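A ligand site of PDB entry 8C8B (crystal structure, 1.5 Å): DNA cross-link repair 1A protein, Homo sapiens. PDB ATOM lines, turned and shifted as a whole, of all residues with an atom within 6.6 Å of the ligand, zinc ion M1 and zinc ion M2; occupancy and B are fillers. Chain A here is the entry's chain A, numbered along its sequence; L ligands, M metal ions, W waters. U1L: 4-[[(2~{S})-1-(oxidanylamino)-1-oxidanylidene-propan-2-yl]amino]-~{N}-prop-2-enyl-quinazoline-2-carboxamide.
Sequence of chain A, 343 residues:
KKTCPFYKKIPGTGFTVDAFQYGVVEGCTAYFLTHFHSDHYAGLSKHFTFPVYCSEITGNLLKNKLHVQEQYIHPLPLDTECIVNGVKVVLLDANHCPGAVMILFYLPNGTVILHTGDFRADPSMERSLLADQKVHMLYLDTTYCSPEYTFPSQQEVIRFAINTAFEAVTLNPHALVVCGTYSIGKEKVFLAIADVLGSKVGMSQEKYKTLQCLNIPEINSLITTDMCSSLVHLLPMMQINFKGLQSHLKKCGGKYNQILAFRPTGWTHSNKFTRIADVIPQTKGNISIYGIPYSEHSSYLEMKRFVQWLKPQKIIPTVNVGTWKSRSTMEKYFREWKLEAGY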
ATOM      1  N   HIS A  35       4.473   4.466  -6.899  1.00  0.00           N
ATOM      2  CA  HIS A  35       4.390   5.392  -5.782  1.00  0.00           C
ATOM      3  C   HIS A  35       3.239   4.997  -4.863  1.00  0.00           C
ATOM      4  O   HIS A  35       2.367   4.211  -5.241  1.00  0.00           O
ATOM      5  CB  HIS A  35       4.247   6.847  -6.243  1.00  0.00           C
ATOM      6  CG  HIS A  35       2.963   7.164  -6.950  1.00  0.00           C
ATOM      7  ND1 HIS A  35       2.632   6.639  -8.182  1.00  0.00           N
ATOM      8  CD2 HIS A  35       1.961   8.003  -6.626  1.00  0.00           C
ATOM      9  CE1 HIS A  35       1.476   7.131  -8.570  1.00  0.00           C
ATOM     10  NE2 HIS A  35       1.041   7.951  -7.638  1.00  0.00           N
ATOM     11  N   PHE A  36       3.250   5.574  -3.654  1.00  0.00           N
ATOM     12  CA  PHE A  36       2.328   5.182  -2.587  1.00  0.00           C
ATOM     13  C   PHE A  36       1.079   6.072  -2.603  1.00  0.00           C
ATOM     14  O   PHE A  36       0.838   6.911  -1.722  1.00  0.00           O
ATOM     15  CB  PHE A  36       3.040   5.226  -1.234  1.00  0.00           C
ATOM     16  CG  PHE A  36       2.274   4.570  -0.107  1.00  0.00           C
ATOM     17  CD1 PHE A  36       2.237   3.190   0.012  1.00  0.00           C
ATOM     18  CD2 PHE A  36       1.604   5.335   0.831  1.00  0.00           C
ATOM     19  CE1 PHE A  36       1.545   2.585   1.048  1.00  0.00           C
ATOM     20  CE2 PHE A  36       0.894   4.746   1.863  1.00  0.00           C
ATOM     21  CZ  PHE A  36       0.869   3.360   1.979  1.00  0.00           C
ATOM     22  N   HIS A  37       0.287   5.903  -3.665  1.00  0.00           N
ATOM     23  CA  HIS A  37      -1.045   6.496  -3.754  1.00  0.00           C
ATOM     24  C   HIS A  37      -2.048   5.371  -3.940  1.00  0.00           C
ATOM     25  O   HIS A  37      -1.800   4.414  -4.693  1.00  0.00           O
ATOM     26  CB  HIS A  37      -1.139   7.495  -4.902  1.00  0.00           C
ATOM     27  CG  HIS A  37      -0.651   8.867  -4.541  1.00  0.00           C
ATOM     28  ND1 HIS A  37      -0.306   9.803  -5.488  1.00  0.00           N
ATOM     29  CD2 HIS A  37      -0.453   9.460  -3.341  1.00  0.00           C
ATOM     30  CE1 HIS A  37       0.073  10.924  -4.899  1.00  0.00           C
ATOM     31  NE2 HIS A  37      -0.008  10.739  -3.591  1.00  0.00           N
ATOM     32  N   SER A  38      -3.189   5.486  -3.246  1.00  0.00           N
ATOM     33  CA  SER A  38      -4.101   4.354  -3.095  1.00  0.00           C
ATOM     34  C   SER A  38      -4.585   3.798  -4.428  1.00  0.00           C
ATOM     35  O   SER A  38      -4.772   2.588  -4.554  1.00  0.00           O
ATOM     36  CB  SER A  38      -5.275   4.721  -2.190  1.00  0.00           C
ATOM     37  OG  SER A  38      -6.071   5.742  -2.757  1.00  0.00           O
ATOM     38  N   ASP A  39      -4.793   4.663  -5.426  1.00  0.00           N
ATOM     39  CA  ASP A  39      -5.211   4.159  -6.736  1.00  0.00           C
ATOM     40  C   ASP A  39      -4.145   3.313  -7.419  1.00  0.00           C
ATOM     41  O   ASP A  39      -4.439   2.657  -8.425  1.00  0.00           O
ATOM     42  CB  ASP A  39      -5.716   5.278  -7.656  1.00  0.00           C
ATOM     43  CG  ASP A  39      -4.810   6.500  -7.654  1.00  0.00           C
ATOM     44  OD1 ASP A  39      -4.342   6.904  -6.567  1.00  0.00           O
ATOM     45  OD2 ASP A  39      -4.578   7.070  -8.746  1.00  0.00           O
ATOM     46  N   HIS A  40      -2.924   3.281  -6.892  1.00  0.00           N
ATOM     47  CA  HIS A  40      -1.843   2.463  -7.448  1.00  0.00           C
ATOM     48  C   HIS A  40      -1.472   1.269  -6.599  1.00  0.00           C
ATOM     49  O   HIS A  40      -1.147   0.215  -7.155  1.00  0.00           O
ATOM     50  CB  HIS A  40      -0.595   3.325  -7.685  1.00  0.00           C
ATOM     51  CG  HIS A  40      -0.855   4.475  -8.587  1.00  0.00           C
ATOM     52  ND1 HIS A  40      -0.361   4.534  -9.878  1.00  0.00           N
ATOM     53  CD2 HIS A  40      -1.610   5.578  -8.422  1.00  0.00           C
ATOM     54  CE1 HIS A  40      -0.786   5.649 -10.449  1.00  0.00           C
ATOM     55  NE2 HIS A  40      -1.543   6.291  -9.588  1.00  0.00           N
ATOM     56  N   HIS A  96       6.522  13.786  -8.650  1.00  0.00           N
ATOM     57  CA  HIS A  96       5.113  13.643  -8.286  1.00  0.00           C
ATOM     58  C   HIS A  96       5.039  13.828  -6.779  1.00  0.00           C
ATOM     59  O   HIS A  96       5.222  14.945  -6.290  1.00  0.00           O
ATOM     60  CB  HIS A  96       4.607  12.299  -8.824  1.00  0.00           C
ATOM     61  CG  HIS A  96       3.152  12.041  -8.591  1.00  0.00           C
ATOM     62  ND1 HIS A  96       2.148  12.891  -9.005  1.00  0.00           N
ATOM     63  CD2 HIS A  96       2.533  11.001  -7.983  1.00  0.00           C
ATOM     64  CE1 HIS A  96       0.980  12.394  -8.661  1.00  0.00           C
ATOM     65  NE2 HIS A  96       1.194  11.251  -8.029  1.00  0.00           N
ATOM     66  N   CYS A  97       4.842  12.764  -6.020  1.00  0.00           N
ATOM     67  CA  CYS A  97       4.871  12.813  -4.563  1.00  0.00           C
ATOM     68  C   CYS A  97       6.150  12.150  -4.051  1.00  0.00           C
ATOM     69  O   CYS A  97       6.925  11.580  -4.828  1.00  0.00           O
ATOM     70  CB  CYS A  97       3.638  12.086  -4.012  1.00  0.00           C
ATOM     71  SG  CYS A  97       3.646  10.314  -4.361  1.00  0.00           S
ATOM     72  N   ASP A 118       2.790   8.163 -12.213  1.00  0.00           N
ATOM     73  CA  ASP A 118       2.319   9.543 -12.209  1.00  0.00           C
ATOM     74  C   ASP A 118       3.520  10.471 -12.170  1.00  0.00           C
ATOM     75  O   ASP A 118       4.476  10.233 -11.428  1.00  0.00           O
ATOM     76  CB  ASP A 118       1.445   9.832 -10.986  1.00  0.00           C
ATOM     77  CG  ASP A 118       0.076   9.226 -11.073  1.00  0.00           C
ATOM     78  OD1 ASP A 118      -0.271   8.703 -12.158  1.00  0.00           O
ATOM     79  OD2 ASP A 118      -0.643   9.283 -10.050  1.00  0.00           O
ATOM     80  N   ASP A 141       1.522   9.181 -18.205  1.00  0.00           N
ATOM     81  CA  ASP A 141       0.514   9.782 -17.333  1.00  0.00           C
ATOM     82  C   ASP A 141      -0.131  10.920 -18.100  1.00  0.00           C
ATOM     83  O   ASP A 141       0.442  12.017 -18.217  1.00  0.00           O
ATOM     84  CB  ASP A 141       1.175  10.262 -16.047  1.00  0.00           C
ATOM     85  CG  ASP A 141       0.273  11.147 -15.190  1.00  0.00           C
ATOM     86  OD1 ASP A 141      -0.949  11.182 -15.428  1.00  0.00           O
ATOM     87  OD2 ASP A 141       0.808  11.833 -14.299  1.00  0.00           O
ATOM     88  N   THR A 143      -3.007  12.480 -17.340  1.00  0.00           N
ATOM     89  CA  THR A 143      -4.069  13.050 -16.509  1.00  0.00           C
ATOM     90  C   THR A 143      -4.624  14.333 -17.112  1.00  0.00           C
ATOM     91  O   THR A 143      -5.839  14.504 -17.230  1.00  0.00           O
ATOM     92  CB  THR A 143      -3.559  13.295 -15.080  1.00  0.00           C
ATOM     93  OG1 THR A 143      -3.228  12.038 -14.475  1.00  0.00           O
ATOM     94  CG2 THR A 143      -4.620  13.979 -14.225  1.00  0.00           C
ATOM     95  N   TYR A 144      -3.747  15.251 -17.509  1.00  0.00           N
ATOM     96  CA  TYR A 144      -4.140  16.573 -17.989  1.00  0.00           C
ATOM     97  C   TYR A 144      -3.756  16.788 -19.451  1.00  0.00           C
ATOM     98  O   TYR A 144      -3.278  17.855 -19.851  1.00  0.00           O
ATOM     99  CB  TYR A 144      -3.538  17.671 -17.113  1.00  0.00           C
ATOM    100  CG  TYR A 144      -4.104  17.701 -15.713  1.00  0.00           C
ATOM    101  CD1 TYR A 144      -5.473  17.720 -15.495  1.00  0.00           C
ATOM    102  CD2 TYR A 144      -3.260  17.711 -14.598  1.00  0.00           C
ATOM    103  CE1 TYR A 144      -5.994  17.762 -14.211  1.00  0.00           C
ATOM    104  CE2 TYR A 144      -3.776  17.736 -13.328  1.00  0.00           C
ATOM    105  CZ  TYR A 144      -5.139  17.765 -13.140  1.00  0.00           C
ATOM    106  OH  TYR A 144      -5.638  17.805 -11.858  1.00  0.00           O
ATOM    107  N   TYR A 182      -5.029  14.487   2.074  1.00  0.00           N
ATOM    108  CA  TYR A 182      -5.639  13.159   2.055  1.00  0.00           C
ATOM    109  C   TYR A 182      -4.688  12.029   1.676  1.00  0.00           C
ATOM    110  O   TYR A 182      -5.064  10.862   1.797  1.00  0.00           O
ATOM    111  CB  TYR A 182      -6.892  13.095   1.163  1.00  0.00           C
ATOM    112  CG  TYR A 182      -6.744  13.686  -0.223  1.00  0.00           C
ATOM    113  CD1 TYR A 182      -5.748  13.256  -1.099  1.00  0.00           C
ATOM    114  CD2 TYR A 182      -7.640  14.643  -0.688  1.00  0.00           C
ATOM    115  CE1 TYR A 182      -5.635  13.783  -2.371  1.00  0.00           C
ATOM    116  CE2 TYR A 182      -7.531  15.179  -1.958  1.00  0.00           C
ATOM    117  CZ  TYR A 182      -6.534  14.751  -2.793  1.00  0.00           C
ATOM    118  OH  TYR A 182      -6.420  15.275  -4.055  1.00  0.00           O
ATOM    119  N   SER A 183      -3.477  12.341   1.217  1.00  0.00           N
ATOM    120  CA  SER A 183      -2.488  11.335   0.838  1.00  0.00           C
ATOM    121  C   SER A 183      -1.131  12.004   0.960  1.00  0.00           C
ATOM    122  O   SER A 183      -1.030  13.181   1.306  1.00  0.00           O
ATOM    123  CB  SER A 183      -2.742  10.868  -0.596  1.00  0.00           C
ATOM    124  OG  SER A 183      -2.781  11.975  -1.482  1.00  0.00           O
ATOM    125  N   ILE A 184      -0.072  11.243   0.665  1.00  0.00           N
ATOM    126  CA  ILE A 184       1.218  11.891   0.554  1.00  0.00           C
ATOM    127  C   ILE A 184       1.256  12.758  -0.700  1.00  0.00           C
ATOM    128  O   ILE A 184       0.422  12.633  -1.603  1.00  0.00           O
ATOM    129  CB  ILE A 184       2.383  10.884   0.566  1.00  0.00           C
ATOM    130  CG1 ILE A 184       2.326   9.978  -0.665  1.00  0.00           C
ATOM    131  CG2 ILE A 184       2.394  10.091   1.860  1.00  0.00           C
ATOM    132  CD1 ILE A 184       3.602   9.164  -0.862  1.00  0.00           C
ATOM    133  N   LYS A 186       2.404  17.043  -1.930  1.00  0.00           N
ATOM    134  CA  LYS A 186       2.028  18.425  -1.660  1.00  0.00           C
ATOM    135  C   LYS A 186       2.439  18.896  -0.274  1.00  0.00           C
ATOM    136  O   LYS A 186       1.919  19.894   0.222  1.00  0.00           O
ATOM    137  CB  LYS A 186       0.539  18.679  -1.944  1.00  0.00           C
ATOM    138  CG  LYS A 186       0.076  18.067  -3.281  1.00  0.00           C
ATOM    139  CD  LYS A 186      -1.347  18.446  -3.660  1.00  0.00           C
ATOM    140  CE  LYS A 186      -1.768  17.728  -4.952  1.00  0.00           C
ATOM    141  NZ  LYS A 186      -3.037  18.275  -5.510  1.00  0.00           N
ATOM    142  N   GLY A 266      -6.177  19.981  -7.589  1.00  0.00           N
ATOM    143  CA  GLY A 266      -5.480  19.845  -8.851  1.00  0.00           C
ATOM    144  C   GLY A 266      -5.819  21.007  -9.742  1.00  0.00           C
ATOM    145  O   GLY A 266      -5.801  22.162  -9.298  1.00  0.00           O
ATOM    146  N   TRP A 267      -6.131  20.738 -11.005  1.00  0.00           N
ATOM    147  CA  TRP A 267      -6.595  21.780 -11.905  1.00  0.00           C
ATOM    148  C   TRP A 267      -8.058  22.080 -11.638  1.00  0.00           C
ATOM    149  O   TRP A 267      -8.853  21.187 -11.349  1.00  0.00           O
ATOM    150  CB  TRP A 267      -6.438  21.327 -13.355  1.00  0.00           C
ATOM    151  CG  TRP A 267      -7.195  22.172 -14.344  1.00  0.00           C
ATOM    152  CD1 TRP A 267      -6.744  23.282 -14.999  1.00  0.00           C
ATOM    153  CD2 TRP A 267      -8.549  21.969 -14.790  1.00  0.00           C
ATOM    154  NE1 TRP A 267      -7.728  23.784 -15.827  1.00  0.00           N
ATOM    155  CE2 TRP A 267      -8.846  22.991 -15.715  1.00  0.00           C
ATOM    156  CE3 TRP A 267      -9.537  21.023 -14.489  1.00  0.00           C
ATOM    157  CZ2 TRP A 267     -10.088  23.093 -16.337  1.00  0.00           C
ATOM    158  CZ3 TRP A 267     -10.766  21.120 -15.114  1.00  0.00           C
ATOM    159  CH2 TRP A 267     -11.034  22.151 -16.030  1.00  0.00           C
ATOM    160  N   GLU A 296       0.667  18.014  -8.812  1.00  0.00           N
ATOM    161  CA  GLU A 296       1.778  17.075  -8.975  1.00  0.00           C
ATOM    162  C   GLU A 296       1.662  16.234 -10.247  1.00  0.00           C
ATOM    163  O   GLU A 296       2.326  15.206 -10.365  1.00  0.00           O
ATOM    164  CB  GLU A 296       1.997  16.241  -7.694  1.00  0.00           C
ATOM    165  CG  GLU A 296       2.625  17.126  -6.587  1.00  0.00           C
ATOM    166  CD  GLU A 296       2.889  16.430  -5.262  1.00  0.00           C
ATOM    167  OE1 GLU A 296       2.352  15.336  -5.014  1.00  0.00           O
ATOM    168  OE2 GLU A 296       3.666  17.007  -4.453  1.00  0.00           O
ATOM    169  N   HIS A 297       0.850  16.691 -11.207  1.00  0.00           N
ATOM    170  CA  HIS A 297       0.793  16.108 -12.545  1.00  0.00           C
ATOM    171  C   HIS A 297       1.185  17.167 -13.564  1.00  0.00           C
ATOM    172  O   HIS A 297       0.974  18.367 -13.331  1.00  0.00           O
ATOM    173  CB  HIS A 297      -0.621  15.622 -12.909  1.00  0.00           C
ATOM    174  CG  HIS A 297      -1.108  14.456 -12.086  1.00  0.00           C
ATOM    175  ND1 HIS A 297      -0.793  13.147 -12.386  1.00  0.00           N
ATOM    176  CD2 HIS A 297      -1.893  14.413 -10.984  1.00  0.00           C
ATOM    177  CE1 HIS A 297      -1.355  12.353 -11.496  1.00  0.00           C
ATOM    178  NE2 HIS A 297      -2.030  13.091 -10.635  1.00  0.00           N
ATOM    179  N   VAL A 319      -4.001   7.141 -18.270  1.00  0.00           N
ATOM    180  CA  VAL A 319      -5.064   7.895 -17.607  1.00  0.00           C
ATOM    181  C   VAL A 319      -6.034   8.394 -18.663  1.00  0.00           C
ATOM    182  O   VAL A 319      -5.647   8.692 -19.798  1.00  0.00           O
ATOM    183  CB  VAL A 319      -4.525   9.073 -16.747  1.00  0.00           C
ATOM    184  CG1 VAL A 319      -5.630   9.758 -15.918  1.00  0.00           C
ATOM    185  CG2 VAL A 319      -3.433   8.582 -15.807  1.00  0.00           C
HETATM  186  C1  U1L L   1      -3.213  11.947  -4.789  1.00  0.00           C
HETATM  187  C10 U1L L   1      -7.888   8.966  -7.351  1.00  0.00           C
HETATM  188  C11 U1L L   1      -6.844  10.589  -8.649  1.00  0.00           C
HETATM  189  C12 U1L L   1      -6.828  11.372  -9.908  1.00  0.00           C
HETATM  190  C13 U1L L   1      -5.954  13.618 -10.316  1.00  0.00           C
HETATM  191  C14 U1L L   1      -6.960  13.992 -11.322  1.00  0.00           C
HETATM  192  C15 U1L L   1      -8.053  14.663 -11.114  1.00  0.00           C
HETATM  193  C2  U1L L   1      -3.873  11.331  -6.011  1.00  0.00           C
HETATM  194  C3  U1L L   1      -2.834  10.671  -6.909  1.00  0.00           C
HETATM  195  C4  U1L L   1      -5.916  10.138  -6.581  1.00  0.00           C
HETATM  196  C5  U1L L   1      -6.932   9.149  -6.326  1.00  0.00           C
HETATM  197  C6  U1L L   1      -7.018   8.372  -5.151  1.00  0.00           C
HETATM  198  C7  U1L L   1      -8.011   7.453  -5.008  1.00  0.00           C
HETATM  199  C8  U1L L   1      -8.958   7.273  -6.033  1.00  0.00           C
HETATM  200  C9  U1L L   1      -8.908   8.006  -7.172  1.00  0.00           C
HETATM  201  N1  U1L L   1      -2.896   9.356  -7.042  1.00  0.00           N
HETATM  202  N2  U1L L   1      -4.953  10.380  -5.648  1.00  0.00           N
HETATM  203  N3  U1L L   1      -7.837   9.694  -8.512  1.00  0.00           N
HETATM  204  N4  U1L L   1      -5.788  12.191 -10.108  1.00  0.00           N
HETATM  205  N5  U1L L   1      -5.905  10.835  -7.723  1.00  0.00           N
HETATM  206  O1  U1L L   1      -1.982   8.696  -7.863  1.00  0.00           O
HETATM  207  O2  U1L L   1      -1.994  11.357  -7.483  1.00  0.00           O
HETATM  208  O3  U1L L   1      -7.785  11.301 -10.683  1.00  0.00           O
HETATM  209 ZN    ZN M   1      -0.318   9.688  -7.701  1.00  0.00          ZN
HETATM  210 ZN    ZN M   2      -2.495   8.301  -9.746  1.00  0.00          ZN
HETATM  211  O   HOH W   1      -3.451  10.387  -9.774  1.00  0.00           O
HETATM  212  O   HOH W   2      -4.487  10.401 -12.527  1.00  0.00           O
HETATM  213  O   HOH W   3      -2.789   8.268 -11.784  1.00  0.00           O
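OD1 of Asp 39 lies within hydrogen-bond range of N1 of the ligand (2.9 Å).
Zinc ion M1 is bound by O1 of the ligand, NE2 of His 96, NE2 of His 35, ND1 of His 37, O2 of the ligand and OD2 of Asp 118.
Zinc ion M1 has six donor atoms within binding distance.
The backbone carbonyl oxygen (O) of Glu 296 sits at hydrogen-bond distance from a ring nitrogen (ND1) of His 96, at 2.7 Å.
NE2 of His 37 sits at hydrogen-bond distance from O of Ile 184 (2.8 Å).
A ring nitrogen (NE2) of His 37 sits close to the side-chain sulfur (SG) of Cys 97 (3.8 Å).
OD2 of Asp 39 sits close to NE2 of His 40, at 3.2 Å.
ND1 of His 297 is in hydrogen-bond range of OG1 of Thr 143, 3.4 Å away.
ND1 of His 297 is in hydrogen-bond range of OD2 of Asp 141 (2.8 Å).
OG1 of Thr 143 is in hydrogen-bond range of OD1 of Asp 141 (2.6 Å).
OG of Ser 38 touches C7 of the ligand, 3.4 Å away.
Thr 143 touches the ligand.
Tyr 182 touches the ligand.
Ser 183 touches the ligand (OG to C1, 3.3 Å).
His 297 touches the ligand (NE2 to O2, 3.6 Å).
Hydrophobic or aromatic side chains within 4 Å of the ligand: His 35, His 37, His 40, His 96 and Tyr 182.
Along chain A the residues within 4 Å of the ligand span positions 35 to 297.
Water W1 lies within hydrogen-bond range of a nitrogen (N4) of the ligand (3.0 Å) and a ring nitrogen (NE2) of His 297 (3.2 Å).
Water W2 lies within hydrogen-bond range of the side-chain hydroxyl of Thr 143 (2.8 Å) and a nitrogen (N4) of the ligand (3.3 Å).
Of the 21 residues printed, 4 come within 4 Å of zinc ion M1.
Three residues have an atom within 4 Å of zinc ion M2: Asp 39, His 40 and Asp 118.
O1 of the ligand binds zinc ion M2 (2.0 Å).
Water W3 binds zinc ion M2 (2.1 Å).
OD2 of Asp 118 is bound to zinc ion M2, 2.1 Å away.
NE2 of His 40 binds zinc ion M2 (2.2 Å).
Zinc ion M2 is bound by water W1, at 2.3 Å.
Zinc ion M2 has five donor atoms within binding distance.
Slightly farther from zinc ion M2 lies the side-chain carboxylate (OD2) of Asp 39 (2.6 Å).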
